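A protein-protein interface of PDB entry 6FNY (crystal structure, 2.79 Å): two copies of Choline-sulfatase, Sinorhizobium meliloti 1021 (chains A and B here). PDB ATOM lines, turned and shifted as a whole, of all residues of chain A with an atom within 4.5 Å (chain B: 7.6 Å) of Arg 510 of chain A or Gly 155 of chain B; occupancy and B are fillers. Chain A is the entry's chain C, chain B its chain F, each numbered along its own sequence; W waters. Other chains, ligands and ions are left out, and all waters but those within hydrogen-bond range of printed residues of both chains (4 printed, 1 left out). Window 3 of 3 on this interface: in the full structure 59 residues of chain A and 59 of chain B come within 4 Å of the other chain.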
ATOM      1  N   GLU A 506      11.934 -34.091  25.654  1.00  0.00           N
ATOM      2  CA  GLU A 506      10.884 -33.798  24.683  1.00  0.00           C
ATOM      3  C   GLU A 506      11.471 -33.404  23.334  1.00  0.00           C
ATOM      4  O   GLU A 506      10.907 -33.734  22.284  1.00  0.00           O
ATOM      5  CB  GLU A 506       9.971 -32.693  25.214  1.00  0.00           C
ATOM      6  CG  GLU A 506       9.106 -33.102  26.396  1.00  0.00           C
ATOM      7  CD  GLU A 506       7.919 -33.957  25.994  1.00  0.00           C
ATOM      8  OE1 GLU A 506       7.276 -34.540  26.893  1.00  0.00           O
ATOM      9  OE2 GLU A 506       7.626 -34.047  24.783  1.00  0.00           O
ATOM     10  N   GLU A 507      12.605 -32.700  23.340  1.00  0.00           N
ATOM     11  CA  GLU A 507      13.231 -32.314  22.079  1.00  0.00           C
ATOM     12  C   GLU A 507      13.859 -33.516  21.384  1.00  0.00           C
ATOM     13  O   GLU A 507      13.785 -33.638  20.155  1.00  0.00           O
ATOM     14  CB  GLU A 507      14.274 -31.222  22.325  1.00  0.00           C
ATOM     15  CG  GLU A 507      15.133 -30.873  21.110  1.00  0.00           C
ATOM     16  CD  GLU A 507      14.419 -29.980  20.104  1.00  0.00           C
ATOM     17  OE1 GLU A 507      13.238 -29.640  20.327  1.00  0.00           O
ATOM     18  OE2 GLU A 507      15.048 -29.613  19.088  1.00  0.00           O
ATOM     19  N   SER A 508      14.471 -34.420  22.154  1.00  0.00           N
ATOM     20  CA  SER A 508      15.127 -35.578  21.554  1.00  0.00           C
ATOM     21  C   SER A 508      14.112 -36.561  20.982  1.00  0.00           C
ATOM     22  O   SER A 508      14.348 -37.160  19.927  1.00  0.00           O
ATOM     23  CB  SER A 508      16.019 -36.266  22.588  1.00  0.00           C
ATOM     24  OG  SER A 508      15.243 -36.911  23.585  1.00  0.00           O
ATOM     25  N   LYS A 509      12.980 -36.741  21.660  1.00  0.00           N
ATOM     26  CA  LYS A 509      11.957 -37.675  21.206  1.00  0.00           C
ATOM     27  C   LYS A 509      11.038 -37.082  20.145  1.00  0.00           C
ATOM     28  O   LYS A 509      10.084 -37.748  19.729  1.00  0.00           O
ATOM     29  CB  LYS A 509      11.126 -38.162  22.395  1.00  0.00           C
ATOM     30  CG  LYS A 509      11.941 -38.850  23.479  1.00  0.00           C
ATOM     31  CD  LYS A 509      12.699 -40.048  22.930  1.00  0.00           C
ATOM     32  CE  LYS A 509      13.765 -40.518  23.906  1.00  0.00           C
ATOM     33  NZ  LYS A 509      14.594 -41.621  23.344  1.00  0.00           N
ATOM     34  N   ARG A 510      11.303 -35.860  19.699  1.00  0.00           N
ATOM     35  CA  ARG A 510      10.471 -35.169  18.726  1.00  0.00           C
ATOM     36  C   ARG A 510      11.191 -35.136  17.386  1.00  0.00           C
ATOM     37  O   ARG A 510      12.384 -34.821  17.329  1.00  0.00           O
ATOM     38  CB  ARG A 510      10.156 -33.750  19.208  1.00  0.00           C
ATOM     39  CG  ARG A 510       9.730 -32.769  18.134  1.00  0.00           C
ATOM     40  CD  ARG A 510       9.598 -31.374  18.726  1.00  0.00           C
ATOM     41  NE  ARG A 510       8.798 -30.489  17.887  1.00  0.00           N
ATOM     42  CZ  ARG A 510       8.308 -29.322  18.291  1.00  0.00           C
ATOM     43  NH1 ARG A 510       8.534 -28.902  19.530  1.00  0.00           N
ATOM     44  NH2 ARG A 510       7.589 -28.579  17.462  1.00  0.00           N
ATOM     45  N   TYR A 511      10.469 -35.484  16.315  1.00  0.00           N
ATOM     46  CA  TYR A 511      11.028 -35.400  14.973  1.00  0.00           C
ATOM     47  C   TYR A 511       9.897 -35.237  13.972  1.00  0.00           C
ATOM     48  O   TYR A 511       8.866 -35.912  14.112  1.00  0.00           O
ATOM     49  CB  TYR A 511      11.865 -36.636  14.625  1.00  0.00           C
ATOM     50  CG  TYR A 511      12.717 -36.446  13.391  1.00  0.00           C
ATOM     51  CD1 TYR A 511      13.987 -35.893  13.480  1.00  0.00           C
ATOM     52  CD2 TYR A 511      12.245 -36.803  12.133  1.00  0.00           C
ATOM     53  CE1 TYR A 511      14.766 -35.710  12.353  1.00  0.00           C
ATOM     54  CE2 TYR A 511      13.017 -36.622  11.001  1.00  0.00           C
ATOM     55  CZ  TYR A 511      14.277 -36.074  11.116  1.00  0.00           C
ATOM     56  OH  TYR A 511      15.050 -35.892   9.992  1.00  0.00           O
ATOM     57  N   PRO A 512      10.037 -34.359  12.964  1.00  0.00           N
ATOM     58  CA  PRO A 512      11.179 -33.454  12.768  1.00  0.00           C
ATOM     59  C   PRO A 512      11.226 -32.326  13.796  1.00  0.00           C
ATOM     60  O   PRO A 512      10.194 -31.967  14.366  1.00  0.00           O
ATOM     61  CB  PRO A 512      10.949 -32.895  11.359  1.00  0.00           C
ATOM     62  CG  PRO A 512      10.026 -33.868  10.702  1.00  0.00           C
ATOM     63  CD  PRO A 512       9.135 -34.350  11.801  1.00  0.00           C
ATOM     64  N   ARG A 513      12.415 -31.785  14.030  1.00  0.00           N
ATOM     65  CA  ARG A 513      12.621 -30.758  15.037  1.00  0.00           C
ATOM     66  C   ARG A 513      12.606 -29.369  14.410  1.00  0.00           C
ATOM     67  O   ARG A 513      12.836 -29.196  13.210  1.00  0.00           O
ATOM     68  CB  ARG A 513      13.944 -30.985  15.773  1.00  0.00           C
ATOM     69  CG  ARG A 513      14.027 -32.331  16.459  1.00  0.00           C
ATOM     70  CD  ARG A 513      15.340 -32.519  17.196  1.00  0.00           C
ATOM     71  NE  ARG A 513      15.472 -33.885  17.693  1.00  0.00           N
ATOM     72  CZ  ARG A 513      15.915 -34.903  16.964  1.00  0.00           C
ATOM     73  NH1 ARG A 513      16.276 -34.709  15.704  1.00  0.00           N
ATOM     74  NH2 ARG A 513      15.999 -36.115  17.495  1.00  0.00           N
ATOM     75  N   GLU A 515      10.118 -27.412  13.880  1.00  0.00           N
ATOM     76  CA  GLU A 515       8.940 -27.080  13.094  1.00  0.00           C
ATOM     77  C   GLU A 515       7.700 -27.041  13.977  1.00  0.00           C
ATOM     78  O   GLU A 515       6.602 -26.755  13.502  1.00  0.00           O
ATOM     79  CB  GLU A 515       8.755 -28.085  11.955  1.00  0.00           C
ATOM     80  CG  GLU A 515       9.750 -27.913  10.818  1.00  0.00           C
ATOM     81  CD  GLU A 515       9.890 -29.160   9.963  1.00  0.00           C
ATOM     82  OE1 GLU A 515      11.039 -29.539   9.648  1.00  0.00           O
ATOM     83  OE2 GLU A 515       8.853 -29.756   9.602  1.00  0.00           O
ATOM     84  N   LEU B 150       6.731 -21.948  29.856  1.00  0.00           N
ATOM     85  CA  LEU B 150       6.066 -21.505  28.639  1.00  0.00           C
ATOM     86  C   LEU B 150       6.813 -21.904  27.370  1.00  0.00           C
ATOM     87  O   LEU B 150       6.420 -21.476  26.279  1.00  0.00           O
ATOM     88  CB  LEU B 150       5.862 -19.989  28.680  1.00  0.00           C
ATOM     89  CG  LEU B 150       4.961 -19.519  29.826  1.00  0.00           C
ATOM     90  CD1 LEU B 150       4.956 -18.003  29.931  1.00  0.00           C
ATOM     91  CD2 LEU B 150       3.546 -20.059  29.657  1.00  0.00           C
ATOM     92  N   GLY B 151       7.875 -22.706  27.486  1.00  0.00           N
ATOM     93  CA  GLY B 151       8.506 -23.265  26.305  1.00  0.00           C
ATOM     94  C   GLY B 151       7.585 -24.155  25.500  1.00  0.00           C
ATOM     95  O   GLY B 151       7.792 -24.324  24.294  1.00  0.00           O
ATOM     96  N   SER B 152       6.565 -24.730  26.145  1.00  0.00           N
ATOM     97  CA  SER B 152       5.555 -25.490  25.418  1.00  0.00           C
ATOM     98  C   SER B 152       4.772 -24.604  24.459  1.00  0.00           C
ATOM     99  O   SER B 152       4.249 -25.091  23.450  1.00  0.00           O
ATOM    100  CB  SER B 152       4.601 -26.172  26.401  1.00  0.00           C
ATOM    101  OG  SER B 152       5.197 -27.315  26.985  1.00  0.00           O
ATOM    102  N   VAL B 153       4.679 -23.310  24.755  1.00  0.00           N
ATOM    103  CA  VAL B 153       3.922 -22.394  23.908  1.00  0.00           C
ATOM    104  C   VAL B 153       4.788 -21.825  22.793  1.00  0.00           C
ATOM    105  O   VAL B 153       4.351 -21.747  21.641  1.00  0.00           O
ATOM    106  CB  VAL B 153       3.302 -21.277  24.767  1.00  0.00           C
ATOM    107  CG1 VAL B 153       2.262 -20.520  23.970  1.00  0.00           C
ATOM    108  CG2 VAL B 153       2.687 -21.860  26.028  1.00  0.00           C
ATOM    109  N   THR B 154       6.019 -21.417  23.109  1.00  0.00           N
ATOM    110  CA  THR B 154       6.917 -20.911  22.079  1.00  0.00           C
ATOM    111  C   THR B 154       7.472 -22.023  21.201  1.00  0.00           C
ATOM    112  O   THR B 154       7.859 -21.759  20.057  1.00  0.00           O
ATOM    113  CB  THR B 154       8.073 -20.130  22.710  1.00  0.00           C
ATOM    114  OG1 THR B 154       8.950 -21.034  23.393  1.00  0.00           O
ATOM    115  CG2 THR B 154       7.546 -19.101  23.698  1.00  0.00           C
ATOM    116  N   GLY B 155       7.520 -23.252  21.704  1.00  0.00           N
ATOM    117  CA  GLY B 155       8.002 -24.391  20.955  1.00  0.00           C
ATOM    118  C   GLY B 155       6.929 -25.223  20.292  1.00  0.00           C
ATOM    119  O   GLY B 155       7.225 -26.329  19.823  1.00  0.00           O
ATOM    120  N   ALA B 156       5.691 -24.739  20.243  1.00  0.00           N
ATOM    121  CA  ALA B 156       4.633 -25.478  19.574  1.00  0.00           C
ATOM    122  C   ALA B 156       4.920 -25.570  18.081  1.00  0.00           C
ATOM    123  O   ALA B 156       5.523 -24.674  17.484  1.00  0.00           O
ATOM    124  CB  ALA B 156       3.280 -24.806  19.814  1.00  0.00           C
ATOM    125  N   GLY B 157       4.490 -26.674  17.475  1.00  0.00           N
ATOM    126  CA  GLY B 157       4.717 -26.865  16.059  1.00  0.00           C
ATOM    127  C   GLY B 157       4.211 -28.181  15.505  1.00  0.00           C
ATOM    128  O   GLY B 157       3.237 -28.752  16.007  1.00  0.00           O
ATOM    129  N   VAL B 158       4.874 -28.668  14.459  1.00  0.00           N
ATOM    130  CA  VAL B 158       4.472 -29.872  13.745  1.00  0.00           C
ATOM    131  C   VAL B 158       5.617 -30.872  13.798  1.00  0.00           C
ATOM    132  O   VAL B 158       6.777 -30.508  13.575  1.00  0.00           O
ATOM    133  CB  VAL B 158       4.092 -29.568  12.284  1.00  0.00           C
ATOM    134  CG1 VAL B 158       3.464 -30.789  11.638  1.00  0.00           C
ATOM    135  CG2 VAL B 158       3.157 -28.373  12.207  1.00  0.00           C
ATOM    136  N   ALA B 159       5.287 -32.127  14.089  1.00  0.00           N
ATOM    137  CA  ALA B 159       6.248 -33.217  14.048  1.00  0.00           C
ATOM    138  C   ALA B 159       5.495 -34.505  13.767  1.00  0.00           C
ATOM    139  O   ALA B 159       4.304 -34.620  14.065  1.00  0.00           O
ATOM    140  CB  ALA B 159       7.044 -33.335  15.353  1.00  0.00           C
ATOM    141  N   GLU B 160       6.197 -35.474  13.184  1.00  0.00           N
ATOM    142  CA  GLU B 160       5.578 -36.752  12.864  1.00  0.00           C
ATOM    143  C   GLU B 160       5.667 -37.756  14.005  1.00  0.00           C
ATOM    144  O   GLU B 160       4.877 -38.708  14.037  1.00  0.00           O
ATOM    145  CB  GLU B 160       6.213 -37.343  11.602  1.00  0.00           C
ATOM    146  CG  GLU B 160       5.843 -36.589  10.337  1.00  0.00           C
ATOM    147  CD  GLU B 160       4.380 -36.177  10.314  1.00  0.00           C
ATOM    148  OE1 GLU B 160       4.104 -34.959  10.374  1.00  0.00           O
ATOM    149  OE2 GLU B 160       3.507 -37.068  10.240  1.00  0.00           O
ATOM    150  N   ILE B 161       6.599 -37.562  14.935  1.00  0.00           N
ATOM    151  CA  ILE B 161       6.702 -38.389  16.132  1.00  0.00           C
ATOM    152  C   ILE B 161       7.078 -37.496  17.305  1.00  0.00           C
ATOM    153  O   ILE B 161       7.817 -36.517  17.147  1.00  0.00           O
ATOM    154  CB  ILE B 161       7.720 -39.539  15.956  1.00  0.00           C
ATOM    155  CG1 ILE B 161       7.520 -40.600  17.042  1.00  0.00           C
ATOM    156  CG2 ILE B 161       9.155 -39.017  15.970  1.00  0.00           C
ATOM    157  CD1 ILE B 161       6.139 -41.215  17.044  1.00  0.00           C
ATOM    158  N   THR B 162       6.535 -37.817  18.477  1.00  0.00           N
ATOM    159  CA  THR B 162       6.880 -37.157  19.726  1.00  0.00           C
ATOM    160  C   THR B 162       6.940 -38.214  20.818  1.00  0.00           C
ATOM    161  O   THR B 162       6.616 -39.385  20.595  1.00  0.00           O
ATOM    162  CB  THR B 162       5.869 -36.063  20.109  1.00  0.00           C
ATOM    163  OG1 THR B 162       4.543 -36.609  20.101  1.00  0.00           O
ATOM    164  CG2 THR B 162       5.938 -34.887  19.144  1.00  0.00           C
ATOM    165  N   ASN B 163       7.356 -37.791  22.013  1.00  0.00           N
ATOM    166  CA  ASN B 163       7.312 -38.695  23.157  1.00  0.00           C
ATOM    167  C   ASN B 163       5.881 -39.088  23.491  1.00  0.00           C
ATOM    168  O   ASN B 163       5.626 -40.227  23.897  1.00  0.00           O
ATOM    169  CB  ASN B 163       7.984 -38.048  24.369  1.00  0.00           C
ATOM    170  CG  ASN B 163       8.079 -38.990  25.557  1.00  0.00           C
ATOM    171  OD1 ASN B 163       8.786 -39.997  25.510  1.00  0.00           O
ATOM    172  ND2 ASN B 163       7.367 -38.663  26.630  1.00  0.00           N
ATOM    173  N   MET B 165       3.240 -39.034  21.257  1.00  0.00           N
ATOM    174  CA  MET B 165       2.588 -39.753  20.168  1.00  0.00           C
ATOM    175  C   MET B 165       3.098 -41.184  20.062  1.00  0.00           C
ATOM    176  O   MET B 165       2.327 -42.092  19.737  1.00  0.00           O
ATOM    177  CB  MET B 165       2.774 -39.009  18.846  1.00  0.00           C
ATOM    178  CG  MET B 165       1.566 -38.169  18.456  1.00  0.00           C
ATOM    179  SD  MET B 165       1.720 -37.375  16.845  1.00  0.00           S
ATOM    180  CE  MET B 165       3.178 -36.370  17.098  1.00  0.00           C
ATOM    181  N   PRO B 206       3.805 -31.101  25.298  1.00  0.00           N
ATOM    182  CA  PRO B 206       3.980 -30.088  24.247  1.00  0.00           C
ATOM    183  C   PRO B 206       2.865 -30.057  23.207  1.00  0.00           C
ATOM    184  O   PRO B 206       2.314 -31.098  22.849  1.00  0.00           O
ATOM    185  CB  PRO B 206       5.305 -30.494  23.592  1.00  0.00           C
ATOM    186  CG  PRO B 206       6.024 -31.257  24.639  1.00  0.00           C
ATOM    187  CD  PRO B 206       4.953 -32.022  25.347  1.00  0.00           C
ATOM    188  N   TYR B 207       2.536 -28.852  22.741  1.00  0.00           N
ATOM    189  CA  TYR B 207       1.500 -28.660  21.727  1.00  0.00           C
ATOM    190  C   TYR B 207       2.130 -28.875  20.354  1.00  0.00           C
ATOM    191  O   TYR B 207       2.434 -27.939  19.612  1.00  0.00           O
ATOM    192  CB  TYR B 207       0.877 -27.275  21.848  1.00  0.00           C
ATOM    193  CG  TYR B 207       0.391 -26.929  23.237  1.00  0.00           C
ATOM    194  CD1 TYR B 207      -0.764 -27.503  23.753  1.00  0.00           C
ATOM    195  CD2 TYR B 207       1.084 -26.022  24.031  1.00  0.00           C
ATOM    196  CE1 TYR B 207      -1.215 -27.188  25.022  1.00  0.00           C
ATOM    197  CE2 TYR B 207       0.638 -25.699  25.302  1.00  0.00           C
ATOM    198  CZ  TYR B 207      -0.512 -26.285  25.791  1.00  0.00           C
ATOM    199  OH  TYR B 207      -0.962 -25.972  27.054  1.00  0.00           O
ATOM    200  N   VAL B 208       2.347 -30.146  20.023  1.00  0.00           N
ATOM    201  CA  VAL B 208       2.899 -30.545  18.734  1.00  0.00           C
ATOM    202  C   VAL B 208       2.042 -31.674  18.182  1.00  0.00           C
ATOM    203  O   VAL B 208       1.706 -32.616  18.909  1.00  0.00           O
ATOM    204  CB  VAL B 208       4.372 -30.985  18.847  1.00  0.00           C
ATOM    205  CG1 VAL B 208       4.964 -31.206  17.467  1.00  0.00           C
ATOM    206  CG2 VAL B 208       5.183 -29.950  19.610  1.00  0.00           C
ATOM    207  N   ALA B 209       1.686 -31.578  16.905  1.00  0.00           N
ATOM    208  CA  ALA B 209       0.828 -32.557  16.259  1.00  0.00           C
ATOM    209  C   ALA B 209       1.432 -32.972  14.925  1.00  0.00           C
ATOM    210  O   ALA B 209       2.401 -32.380  14.441  1.00  0.00           O
ATOM    211  CB  ALA B 209      -0.588 -32.005  16.051  1.00  0.00           C
ATOM    212  N   PHE B 251      10.186 -15.638  28.881  1.00  0.00           N
ATOM    213  CA  PHE B 251       9.473 -16.047  27.678  1.00  0.00           C
ATOM    214  C   PHE B 251       8.672 -14.867  27.151  1.00  0.00           C
ATOM    215  O   PHE B 251       7.921 -14.239  27.903  1.00  0.00           O
ATOM    216  CB  PHE B 251       8.550 -17.240  27.954  1.00  0.00           C
ATOM    217  CG  PHE B 251       9.280 -18.536  28.170  1.00  0.00           C
ATOM    218  CD1 PHE B 251       9.810 -19.236  27.101  1.00  0.00           C
ATOM    219  CD2 PHE B 251       9.437 -19.053  29.445  1.00  0.00           C
ATOM    220  CE1 PHE B 251      10.484 -20.427  27.299  1.00  0.00           C
ATOM    221  CE2 PHE B 251      10.109 -20.243  29.649  1.00  0.00           C
ATOM    222  CZ  PHE B 251      10.633 -20.931  28.573  1.00  0.00           C
ATOM    223  N   ASN B 257       2.584 -17.518  18.772  1.00  0.00           N
ATOM    224  CA  ASN B 257       2.834 -18.607  19.711  1.00  0.00           C
ATOM    225  C   ASN B 257       1.542 -19.106  20.346  1.00  0.00           C
ATOM    226  O   ASN B 257       1.417 -20.300  20.643  1.00  0.00           O
ATOM    227  CB  ASN B 257       3.812 -18.155  20.797  1.00  0.00           C
ATOM    228  CG  ASN B 257       5.212 -17.922  20.263  1.00  0.00           C
ATOM    229  OD1 ASN B 257       5.939 -17.055  20.752  1.00  0.00           O
ATOM    230  ND2 ASN B 257       5.598 -18.696  19.259  1.00  0.00           N
ATOM    231  N   ARG B 260      -0.533 -21.054  17.368  1.00  0.00           N
ATOM    232  CA  ARG B 260       0.070 -22.338  17.024  1.00  0.00           C
ATOM    233  C   ARG B 260      -0.122 -23.354  18.141  1.00  0.00           C
ATOM    234  O   ARG B 260      -0.396 -24.531  17.881  1.00  0.00           O
ATOM    235  CB  ARG B 260       1.556 -22.154  16.714  1.00  0.00           C
ATOM    236  CG  ARG B 260       1.832 -21.196  15.567  1.00  0.00           C
ATOM    237  CD  ARG B 260       2.900 -21.741  14.639  1.00  0.00           C
ATOM    238  NE  ARG B 260       4.084 -22.173  15.373  1.00  0.00           N
ATOM    239  CZ  ARG B 260       4.985 -23.025  14.896  1.00  0.00           C
ATOM    240  NH1 ARG B 260       4.835 -23.538  13.682  1.00  0.00           N
ATOM    241  NH2 ARG B 260       6.034 -23.364  15.634  1.00  0.00           N
ATOM    242  N   SER B 261       0.015 -22.914  19.395  1.00  0.00           N
ATOM    243  CA  SER B 261      -0.191 -23.816  20.522  1.00  0.00           C
ATOM    244  C   SER B 261      -1.637 -24.283  20.596  1.00  0.00           C
ATOM    245  O   SER B 261      -1.902 -25.469  20.823  1.00  0.00           O
ATOM    246  CB  SER B 261       0.221 -23.131  21.822  1.00  0.00           C
ATOM    247  OG  SER B 261       1.555 -22.663  21.738  1.00  0.00           O
HETATM  248  O   HOH W   1       5.515 -25.037  11.309  1.00  0.00           O
HETATM  249  O   HOH W   2       7.068 -31.919  10.747  1.00  0.00           O
HETATM  250  O   HOH W   3       5.731 -35.326  23.740  1.00  0.00           O
HETATM  251  O   HOH W   4       8.596 -35.459  22.543  1.00  0.00           O
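The backbone carbonyl oxygen (O) of Tyr 511 of chain A sits at hydrogen-bond distance from the backbone NH (N) of Glu 160 of chain B (2.9 Å). NH1 of Arg 510 of chain A lies within hydrogen-bond range of O of Gly 155 of chain B (2.9 Å). N of Ile 161 of chain B lies within hydrogen-bond range of O of Tyr 511 of chain A (2.9 Å). N of Val 158 of chain B sits at hydrogen-bond distance from O of Glu 515 of chain A (2.7 Å).
The backbone carbonyl oxygen (O) of Gly 157 of chain B is in hydrogen-bond range of the backbone NH (N) of Ala 209 of chain B, at 3.3 Å. O of Arg 510 of chain A sits close to NE of Arg 513 of chain A (3.2 Å). N of Ala 159 of chain B is in hydrogen-bond range of O of Ala 209 of chain B. The backbone NH (N) of Gly 157 of chain B sits at hydrogen-bond distance from the backbone carbonyl oxygen (O) of Tyr 207 of chain B (3.2 Å). The side-chain hydroxyl (OG1) of Thr 162 of chain B lies within hydrogen-bond range of the backbone NH (N) of Met 165 of chain B (3.0 Å).
Among the printed residues, pairs that only touch across the chains: Glu 506 of chain A with Pro 206 of chain B, Lys 509 of chain A with Ile 161 of chain B, Lys 509 of chain A with Thr 162 of chain B, Lys 509 of chain A with Asn 163 of chain B, Arg 510 of chain A with Gly 157 of chain B, Arg 510 of chain A with Ala 159 of chain B, Arg 510 of chain A with Ile 161 of chain B, Arg 510 of chain A with Val 208 of chain B, Tyr 511 of chain A with Ala 159 of chain B, Pro 512 of chain A with Val 158 of chain B, Pro 512 of chain A with Ala 159 of chain B, Pro 512 of chain A with Glu 160 of chain B, Glu 515 of chain A with Gly 157 of chain B and Glu 515 of chain A with Arg 260 of chain B.
Of the printed residues of chain B, Lys 509 of chain A touches Ile 161 (3.6 Å), Thr 162 (3.3 Å) and Asn 163 (3.6 Å). Ser 152 of chain B touches none of the printed residues of chain A. Of the printed residues of chain A, Asn 163 of chain B touches Lys 509. Phe 251 of chain B touches none of the printed residues of chain A. The nearest printed residue of chain B that does not touch Arg 510 of chain A is Val 158 of chain B (4.05 Å). The nearest printed residue of chain A that does not touch Pro 206 of chain B is Arg 510 of chain A (5.4 Å).
Of the 9 printed residues of chain A, 6 touch a printed residue of chain B. Hydrophobic or aromatic side chains of chain A that line the printed part of chain B: Tyr 511 and Pro 512. Printed residues of chain B that touch a printed residue of chain A: Gly 155, Gly 157, Val 158, Ala 159, Glu 160, Ile 161, Thr 162, Asn 163, Pro 206, Val 208 and Arg 260. Among the printed residues, no Asp or Glu carboxylate lies within 4 Å of a Lys or Arg side-chain nitrogen of the other chain.
No position is printed for both chains.
Water W3 lies within hydrogen-bond range of OE2 of Glu 506 of chain A and N of Asn 163 of chain B. Water W4 bridges N of Asn 163 of chain B and OE2 of Glu 506 of chain A. Water W1 lies within hydrogen-bond range of NH1 of Arg 260 of chain B (2.9 Å) and O of Glu 515 of chain A (3.0 Å). Water W2 lies within hydrogen-bond range of OE2 of Glu 515 of chain A (3.0 Å) and O of Val 158 of chain B (3.2 Å).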
